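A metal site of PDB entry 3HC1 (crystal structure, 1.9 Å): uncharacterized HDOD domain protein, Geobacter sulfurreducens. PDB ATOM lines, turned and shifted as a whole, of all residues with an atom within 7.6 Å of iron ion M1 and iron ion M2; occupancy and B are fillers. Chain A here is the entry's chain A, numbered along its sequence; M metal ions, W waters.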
ATOM      1  N   LEU A 119      -8.625  -0.879  13.979  1.00  0.00           N
ATOM      2  CA  LEU A 119      -8.601  -1.386  15.340  1.00  0.00           C
ATOM      3  C   LEU A 119      -9.824  -0.917  16.119  1.00  0.00           C
ATOM      4  O   LEU A 119     -10.401  -1.687  16.854  1.00  0.00           O
ATOM      5  CB  LEU A 119      -7.284  -1.005  16.046  1.00  0.00           C
ATOM      6  CG  LEU A 119      -6.141  -2.007  15.749  1.00  0.00           C
ATOM      7  CD1 LEU A 119      -5.825  -2.168  14.252  1.00  0.00           C
ATOM      8  CD2 LEU A 119      -4.889  -1.627  16.514  1.00  0.00           C
ATOM      9  N   HIS A 122     -13.212  -2.717  14.794  1.00  0.00           N
ATOM     10  CA  HIS A 122     -13.216  -4.107  15.275  1.00  0.00           C
ATOM     11  C   HIS A 122     -13.508  -4.198  16.792  1.00  0.00           C
ATOM     12  O   HIS A 122     -14.276  -5.067  17.258  1.00  0.00           O
ATOM     13  CB  HIS A 122     -11.854  -4.753  14.981  1.00  0.00           C
ATOM     14  CG  HIS A 122     -11.661  -6.073  15.668  1.00  0.00           C
ATOM     15  ND1 HIS A 122     -12.423  -7.181  15.359  1.00  0.00           N
ATOM     16  CD2 HIS A 122     -10.847  -6.450  16.682  1.00  0.00           C
ATOM     17  CE1 HIS A 122     -12.031  -8.203  16.105  1.00  0.00           C
ATOM     18  NE2 HIS A 122     -11.089  -7.779  16.933  1.00  0.00           N
ATOM     19  N   SER A 123     -12.880  -3.310  17.558  1.00  0.00           N
ATOM     20  CA  SER A 123     -13.030  -3.275  19.010  1.00  0.00           C
ATOM     21  C   SER A 123     -14.444  -2.877  19.418  1.00  0.00           C
ATOM     22  O   SER A 123     -15.058  -3.540  20.305  1.00  0.00           O
ATOM     23  CB  SER A 123     -11.984  -2.358  19.656  1.00  0.00           C
ATOM     24  OG  SER A 123     -10.657  -2.872  19.458  1.00  0.00           O
ATOM     25  N   VAL A 126     -16.795  -5.877  18.519  1.00  0.00           N
ATOM     26  CA  VAL A 126     -16.657  -6.875  19.551  1.00  0.00           C
ATOM     27  C   VAL A 126     -17.378  -6.470  20.862  1.00  0.00           C
ATOM     28  O   VAL A 126     -18.111  -7.289  21.435  1.00  0.00           O
ATOM     29  CB  VAL A 126     -15.171  -7.285  19.783  1.00  0.00           C
ATOM     30  CG1 VAL A 126     -14.980  -8.217  21.076  1.00  0.00           C
ATOM     31  CG2 VAL A 126     -14.662  -8.003  18.496  1.00  0.00           C
ATOM     32  N   GLY A 149     -14.931  -6.282  26.156  1.00  0.00           N
ATOM     33  CA  GLY A 149     -14.901  -6.393  24.697  1.00  0.00           C
ATOM     34  C   GLY A 149     -14.166  -5.269  24.000  1.00  0.00           C
ATOM     35  O   GLY A 149     -13.289  -5.481  23.148  1.00  0.00           O
ATOM     36  N   HIS A 152     -10.440  -5.639  24.546  1.00  0.00           N
ATOM     37  CA  HIS A 152      -9.821  -6.960  24.309  1.00  0.00           C
ATOM     38  C   HIS A 152      -8.483  -6.970  23.528  1.00  0.00           C
ATOM     39  O   HIS A 152      -7.552  -7.696  23.840  1.00  0.00           O
ATOM     40  CB  HIS A 152     -10.810  -7.987  23.749  1.00  0.00           C
ATOM     41  CG  HIS A 152     -10.980  -7.917  22.256  1.00  0.00           C
ATOM     42  ND1 HIS A 152     -11.684  -6.911  21.645  1.00  0.00           N
ATOM     43  CD2 HIS A 152     -10.548  -8.723  21.243  1.00  0.00           C
ATOM     44  CE1 HIS A 152     -11.632  -7.059  20.332  1.00  0.00           C
ATOM     45  NE2 HIS A 152     -10.975  -8.166  20.063  1.00  0.00           N
ATOM     46  N   ASP A 153      -8.428  -6.121  22.501  1.00  0.00           N
ATOM     47  CA  ASP A 153      -7.286  -5.934  21.662  1.00  0.00           C
ATOM     48  C   ASP A 153      -6.452  -4.704  21.997  1.00  0.00           C
ATOM     49  O   ASP A 153      -5.692  -4.213  21.130  1.00  0.00           O
ATOM     50  CB  ASP A 153      -7.750  -5.895  20.204  1.00  0.00           C
ATOM     51  CG  ASP A 153      -7.884  -7.303  19.617  1.00  0.00           C
ATOM     52  OD1 ASP A 153      -7.347  -8.245  20.236  1.00  0.00           O
ATOM     53  OD2 ASP A 153      -8.551  -7.457  18.561  1.00  0.00           O
ATOM     54  N   VAL A 154      -6.548  -4.213  23.235  1.00  0.00           N
ATOM     55  CA  VAL A 154      -5.759  -3.033  23.615  1.00  0.00           C
ATOM     56  C   VAL A 154      -4.234  -3.282  23.408  1.00  0.00           C
ATOM     57  O   VAL A 154      -3.484  -2.374  23.127  1.00  0.00           O
ATOM     58  CB  VAL A 154      -6.091  -2.572  25.064  1.00  0.00           C
ATOM     59  CG1 VAL A 154      -5.569  -3.585  26.108  1.00  0.00           C
ATOM     60  CG2 VAL A 154      -5.566  -1.240  25.322  1.00  0.00           C
ATOM     61  N   GLU A 156      -2.886  -4.816  20.764  1.00  0.00           N
ATOM     62  CA  GLU A 156      -2.614  -4.525  19.327  1.00  0.00           C
ATOM     63  C   GLU A 156      -2.529  -3.041  19.139  1.00  0.00           C
ATOM     64  O   GLU A 156      -1.755  -2.570  18.321  1.00  0.00           O
ATOM     65  CB  GLU A 156      -3.692  -5.049  18.367  1.00  0.00           C
ATOM     66  CG  GLU A 156      -3.877  -6.508  18.281  1.00  0.00           C
ATOM     67  CD  GLU A 156      -2.769  -7.211  17.498  1.00  0.00           C
ATOM     68  OE1 GLU A 156      -1.601  -6.993  17.833  1.00  0.00           O
ATOM     69  OE2 GLU A 156      -3.095  -7.978  16.574  1.00  0.00           O
ATOM     70  N   PHE A 181      -2.613 -12.805  13.119  1.00  0.00           N
ATOM     71  CA  PHE A 181      -1.743 -11.820  13.739  1.00  0.00           C
ATOM     72  C   PHE A 181      -1.135 -12.426  14.981  1.00  0.00           C
ATOM     73  O   PHE A 181       0.039 -12.263  15.215  1.00  0.00           O
ATOM     74  CB  PHE A 181      -2.529 -10.556  14.067  1.00  0.00           C
ATOM     75  CG  PHE A 181      -2.454  -9.521  12.964  1.00  0.00           C
ATOM     76  CD1 PHE A 181      -3.093  -9.731  11.751  1.00  0.00           C
ATOM     77  CD2 PHE A 181      -1.787  -8.323  13.180  1.00  0.00           C
ATOM     78  CE1 PHE A 181      -3.037  -8.769  10.744  1.00  0.00           C
ATOM     79  CE2 PHE A 181      -1.725  -7.368  12.170  1.00  0.00           C
ATOM     80  CZ  PHE A 181      -2.366  -7.576  10.981  1.00  0.00           C
ATOM     81  N   GLY A 182      -1.942 -13.127  15.775  1.00  0.00           N
ATOM     82  CA  GLY A 182      -1.445 -13.754  16.973  1.00  0.00           C
ATOM     83  C   GLY A 182      -0.309 -14.749  16.679  1.00  0.00           C
ATOM     84  O   GLY A 182       0.656 -14.828  17.450  1.00  0.00           O
ATOM     85  N   GLU A 185       2.748 -12.657  15.579  1.00  0.00           N
ATOM     86  CA  GLU A 185       3.332 -12.077  16.766  1.00  0.00           C
ATOM     87  C   GLU A 185       4.169 -13.119  17.544  1.00  0.00           C
ATOM     88  O   GLU A 185       5.292 -12.860  17.990  1.00  0.00           O
ATOM     89  CB  GLU A 185       2.216 -11.471  17.657  1.00  0.00           C
ATOM     90  CG  GLU A 185       1.658 -10.212  17.045  1.00  0.00           C
ATOM     91  CD  GLU A 185       0.340  -9.788  17.627  1.00  0.00           C
ATOM     92  OE1 GLU A 185      -0.160 -10.384  18.632  1.00  0.00           O
ATOM     93  OE2 GLU A 185      -0.243  -8.901  16.991  1.00  0.00           O
ATOM     94  N   SER A 192       2.365 -12.446  22.408  1.00  0.00           N
ATOM     95  CA  SER A 192       1.360 -11.803  21.576  1.00  0.00           C
ATOM     96  C   SER A 192       0.679 -10.589  22.244  1.00  0.00           C
ATOM     97  O   SER A 192       0.948 -10.263  23.414  1.00  0.00           O
ATOM     98  CB  SER A 192       0.307 -12.846  21.183  1.00  0.00           C
ATOM     99  OG  SER A 192      -0.744 -12.887  22.148  1.00  0.00           O
ATOM    100  N   HIS A 193      -0.225  -9.961  21.516  1.00  0.00           N
ATOM    101  CA  HIS A 193      -1.030  -8.865  22.057  1.00  0.00           C
ATOM    102  C   HIS A 193      -1.900  -9.287  23.240  1.00  0.00           C
ATOM    103  O   HIS A 193      -2.332  -8.399  24.019  1.00  0.00           O
ATOM    104  CB  HIS A 193      -1.920  -8.217  20.990  1.00  0.00           C
ATOM    105  CG  HIS A 193      -3.002  -9.108  20.482  1.00  0.00           C
ATOM    106  ND1 HIS A 193      -2.758 -10.174  19.636  1.00  0.00           N
ATOM    107  CD2 HIS A 193      -4.323  -9.133  20.739  1.00  0.00           C
ATOM    108  CE1 HIS A 193      -3.892 -10.786  19.367  1.00  0.00           C
ATOM    109  NE2 HIS A 193      -4.861 -10.149  20.007  1.00  0.00           N
ATOM    110  N   CYS A 194      -2.197 -10.579  23.375  1.00  0.00           N
ATOM    111  CA  CYS A 194      -2.859 -11.126  24.580  1.00  0.00           C
ATOM    112  C   CYS A 194      -2.031 -10.853  25.816  1.00  0.00           C
ATOM    113  O   CYS A 194      -2.498 -10.263  26.765  1.00  0.00           O
ATOM    114  CB  CYS A 194      -3.114 -12.598  24.462  1.00  0.00           C
ATOM    115  SG  CYS A 194      -4.238 -13.052  23.112  1.00  0.00           S
ATOM    116  N   ILE A 214      -8.486 -10.073  28.098  1.00  0.00           N
ATOM    117  CA  ILE A 214      -7.382  -9.651  27.168  1.00  0.00           C
ATOM    118  C   ILE A 214      -6.387 -10.811  26.963  1.00  0.00           C
ATOM    119  O   ILE A 214      -6.036 -11.105  25.840  1.00  0.00           O
ATOM    120  CB  ILE A 214      -6.716  -8.372  27.690  1.00  0.00           C
ATOM    121  CG1 ILE A 214      -7.688  -7.200  27.777  1.00  0.00           C
ATOM    122  CG2 ILE A 214      -5.515  -7.940  26.795  1.00  0.00           C
ATOM    123  CD1 ILE A 214      -7.101  -6.022  28.638  1.00  0.00           C
ATOM    124  N   HIS A 217      -8.631 -14.280  25.229  1.00  0.00           N
ATOM    125  CA  HIS A 217      -9.683 -14.109  24.238  1.00  0.00           C
ATOM    126  C   HIS A 217      -9.506 -14.869  22.950  1.00  0.00           C
ATOM    127  O   HIS A 217     -10.501 -15.034  22.229  1.00  0.00           O
ATOM    128  CB  HIS A 217      -9.998 -12.654  23.963  1.00  0.00           C
ATOM    129  CG  HIS A 217      -8.953 -11.930  23.165  1.00  0.00           C
ATOM    130  ND1 HIS A 217      -7.969 -11.152  23.742  1.00  0.00           N
ATOM    131  CD2 HIS A 217      -8.826 -11.769  21.826  1.00  0.00           C
ATOM    132  CE1 HIS A 217      -7.236 -10.606  22.784  1.00  0.00           C
ATOM    133  NE2 HIS A 217      -7.681 -11.041  21.625  1.00  0.00           N
ATOM    134  N   HIS A 218      -8.291 -15.337  22.652  1.00  0.00           N
ATOM    135  CA  HIS A 218      -8.053 -16.211  21.472  1.00  0.00           C
ATOM    136  C   HIS A 218      -8.112 -17.700  21.802  1.00  0.00           C
ATOM    137  O   HIS A 218      -7.994 -18.500  20.903  1.00  0.00           O
ATOM    138  CB  HIS A 218      -6.734 -15.844  20.736  1.00  0.00           C
ATOM    139  CG  HIS A 218      -6.802 -14.545  20.011  1.00  0.00           C
ATOM    140  ND1 HIS A 218      -7.460 -14.420  18.805  1.00  0.00           N
ATOM    141  CD2 HIS A 218      -6.319 -13.299  20.305  1.00  0.00           C
ATOM    142  CE1 HIS A 218      -7.429 -13.148  18.423  1.00  0.00           C
ATOM    143  NE2 HIS A 218      -6.724 -12.447  19.292  1.00  0.00           N
ATOM    144  N   VAL A 234     -16.658 -12.505  24.963  1.00  0.00           N
ATOM    145  CA  VAL A 234     -15.757 -11.657  24.156  1.00  0.00           C
ATOM    146  C   VAL A 234     -14.986 -12.536  23.184  1.00  0.00           C
ATOM    147  O   VAL A 234     -14.771 -12.121  22.022  1.00  0.00           O
ATOM    148  CB  VAL A 234     -14.822 -10.826  25.060  1.00  0.00           C
ATOM    149  CG1 VAL A 234     -13.600 -10.140  24.249  1.00  0.00           C
ATOM    150  CG2 VAL A 234     -15.637  -9.799  25.924  1.00  0.00           C
ATOM    151  N   ALA A 237     -17.421 -13.196  20.434  1.00  0.00           N
ATOM    152  CA  ALA A 237     -17.626 -11.962  19.670  1.00  0.00           C
ATOM    153  C   ALA A 237     -16.446 -11.617  18.756  1.00  0.00           C
ATOM    154  O   ALA A 237     -16.638 -11.144  17.638  1.00  0.00           O
ATOM    155  CB  ALA A 237     -18.011 -10.784  20.582  1.00  0.00           C
ATOM    156  N   ASP A 238     -15.232 -11.902  19.201  1.00  0.00           N
ATOM    157  CA  ASP A 238     -14.065 -11.610  18.417  1.00  0.00           C
ATOM    158  C   ASP A 238     -14.009 -12.515  17.186  1.00  0.00           C
ATOM    159  O   ASP A 238     -13.841 -12.040  16.051  1.00  0.00           O
ATOM    160  CB  ASP A 238     -12.774 -11.748  19.234  1.00  0.00           C
ATOM    161  CG  ASP A 238     -11.569 -11.668  18.378  1.00  0.00           C
ATOM    162  OD1 ASP A 238     -11.427 -10.643  17.717  1.00  0.00           O
ATOM    163  OD2 ASP A 238     -10.776 -12.624  18.294  1.00  0.00           O
ATOM    164  N   GLU A 239     -14.165 -13.816  17.399  1.00  0.00           N
ATOM    165  CA  GLU A 239     -14.184 -14.758  16.285  1.00  0.00           C
ATOM    166  C   GLU A 239     -15.337 -14.450  15.288  1.00  0.00           C
ATOM    167  O   GLU A 239     -15.137 -14.439  14.060  1.00  0.00           O
ATOM    168  CB  GLU A 239     -14.212 -16.213  16.794  1.00  0.00           C
ATOM    169  CG  GLU A 239     -13.930 -17.189  15.644  1.00  0.00           C
ATOM    170  CD  GLU A 239     -13.524 -18.543  16.077  1.00  0.00           C
ATOM    171  OE1 GLU A 239     -13.799 -18.837  17.230  1.00  0.00           O
ATOM    172  OE2 GLU A 239     -12.914 -19.305  15.287  1.00  0.00           O
ATOM    173  N   CYS A 241     -16.837 -11.442  14.734  1.00  0.00           N
ATOM    174  CA  CYS A 241     -16.451 -10.237  14.023  1.00  0.00           C
ATOM    175  C   CYS A 241     -15.390 -10.506  12.970  1.00  0.00           C
ATOM    176  O   CYS A 241     -15.503 -10.017  11.864  1.00  0.00           O
ATOM    177  CB  CYS A 241     -16.007  -9.170  14.980  1.00  0.00           C
ATOM    178  SG  CYS A 241     -17.442  -8.429  15.835  1.00  0.00           S
ATOM    179  N   THR A 242     -14.386 -11.330  13.306  1.00  0.00           N
ATOM    180  CA  THR A 242     -13.296 -11.639  12.388  1.00  0.00           C
ATOM    181  C   THR A 242     -13.837 -12.393  11.187  1.00  0.00           C
ATOM    182  O   THR A 242     -13.407 -12.148  10.069  1.00  0.00           O
ATOM    183  CB  THR A 242     -12.198 -12.434  13.099  1.00  0.00           C
ATOM    184  OG1 THR A 242     -11.749 -11.648  14.208  1.00  0.00           O
ATOM    185  CG2 THR A 242     -10.982 -12.728  12.165  1.00  0.00           C
ATOM    186  N   LEU A 246     -15.724  -7.774  10.238  1.00  0.00           N
ATOM    187  CA  LEU A 246     -15.582  -6.698  11.217  1.00  0.00           C
ATOM    188  C   LEU A 246     -14.277  -6.920  12.023  1.00  0.00           C
ATOM    189  O   LEU A 246     -14.259  -6.913  13.240  1.00  0.00           O
ATOM    190  CB  LEU A 246     -16.839  -6.626  12.084  1.00  0.00           C
ATOM    191  CG  LEU A 246     -17.100  -5.473  13.073  1.00  0.00           C
ATOM    192  CD1 LEU A 246     -16.733  -4.143  12.444  1.00  0.00           C
ATOM    193  CD2 LEU A 246     -18.538  -5.544  13.552  1.00  0.00           C
ATOM    194  N   GLY A 247     -13.201  -7.207  11.303  1.00  0.00           N
ATOM    195  CA  GLY A 247     -11.918  -7.522  11.920  1.00  0.00           C
ATOM    196  C   GLY A 247     -10.723  -7.474  11.007  1.00  0.00           C
ATOM    197  O   GLY A 247     -10.795  -7.030   9.823  1.00  0.00           O
ATOM    198  N   PHE A 248      -9.597  -7.877  11.556  1.00  0.00           N
ATOM    199  CA  PHE A 248      -8.336  -7.767  10.798  1.00  0.00           C
ATOM    200  C   PHE A 248      -7.337  -8.833  11.167  1.00  0.00           C
ATOM    201  O   PHE A 248      -6.290  -8.899  10.561  1.00  0.00           O
ATOM    202  CB  PHE A 248      -7.677  -6.372  11.059  1.00  0.00           C
ATOM    203  CG  PHE A 248      -7.252  -6.165  12.503  1.00  0.00           C
ATOM    204  CD1 PHE A 248      -8.173  -5.779  13.438  1.00  0.00           C
ATOM    205  CD2 PHE A 248      -5.933  -6.422  12.925  1.00  0.00           C
ATOM    206  CE1 PHE A 248      -7.817  -5.627  14.814  1.00  0.00           C
ATOM    207  CE2 PHE A 248      -5.557  -6.276  14.254  1.00  0.00           C
ATOM    208  CZ  PHE A 248      -6.500  -5.875  15.206  1.00  0.00           C
ATOM    209  N   GLU A 249      -7.583  -9.589  12.251  1.00  0.00           N
ATOM    210  CA  GLU A 249      -6.526 -10.408  12.811  1.00  0.00           C
ATOM    211  C   GLU A 249      -6.350 -11.698  12.055  1.00  0.00           C
ATOM    212  O   GLU A 249      -5.385 -12.399  12.281  1.00  0.00           O
ATOM    213  CB  GLU A 249      -6.804 -10.682  14.304  1.00  0.00           C
ATOM    214  CG  GLU A 249      -6.717  -9.417  15.163  1.00  0.00           C
ATOM    215  CD  GLU A 249      -7.447  -9.602  16.440  1.00  0.00           C
ATOM    216  OE1 GLU A 249      -8.672  -9.588  16.408  1.00  0.00           O
ATOM    217  OE2 GLU A 249      -6.784  -9.828  17.470  1.00  0.00           O
HETATM  218 FE    FE M   1      -9.870  -9.096  18.239  1.00  0.00          FE
HETATM  219 FE    FE M   2      -7.121 -10.320  19.635  1.00  0.00          FE
HETATM  220  O   HOH W   1      -8.953 -10.557  19.217  1.00  0.00           O
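O of His 152 sits close to ND1 of His 217 (3.5 Å).
A ring nitrogen (ND1) of His 217 sits at hydrogen-bond distance from the backbone carbonyl oxygen (O) of Ile 214, 2.9 Å away.
ND1 of His 122 lies within hydrogen-bond range of O of Leu 246, 2.8 Å away.
The backbone carbonyl oxygen of Glu 249 is in hydrogen-bond range of the backbone NH of Phe 181 (2.9 Å).
O of Asp 238 sits at hydrogen-bond distance from OG1 of Thr 242 (2.8 Å).
OE1 of Glu 185 sits at hydrogen-bond distance from ND1 of His 193, 2.8 Å away.
The backbone carbonyl oxygen (O) of Gly 149 lies within hydrogen-bond range of a ring nitrogen (ND1) of His 152 (2.6 Å).
Within 4 Å of iron ion M1: His 122, His 152, Asp 153, Asp 238 and Glu 249.
Within 4 Å of iron ion M2: Asp 153, His 193, His 217, His 218 and Glu 249.
The nearest printed residue that does not touch iron ion M2 is His 152 (4.1 Å).
Iron ion M1 is bound by water W1, the side-chain carboxylate (OD2) of Asp 153, a ring nitrogen (NE2) of His 122, the side-chain carboxylate (OE1) of Glu 249, the side-chain carboxylate (OD1) of Asp 238 and a ring nitrogen (NE2) of His 152.
Iron ion M1 has six donor atoms within binding distance.
Iron ion M2 is bound by water W1 (1.9 Å), the side-chain carboxylate (OD1) of Asp 153 (2.2 Å), a ring nitrogen (NE2) of His 217 (2.2 Å), a ring nitrogen (NE2) of His 218 (2.2 Å), the side-chain carboxylate (OE2) of Glu 249 (2.2 Å) and a ring nitrogen (NE2) of His 193 (2.3 Å).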
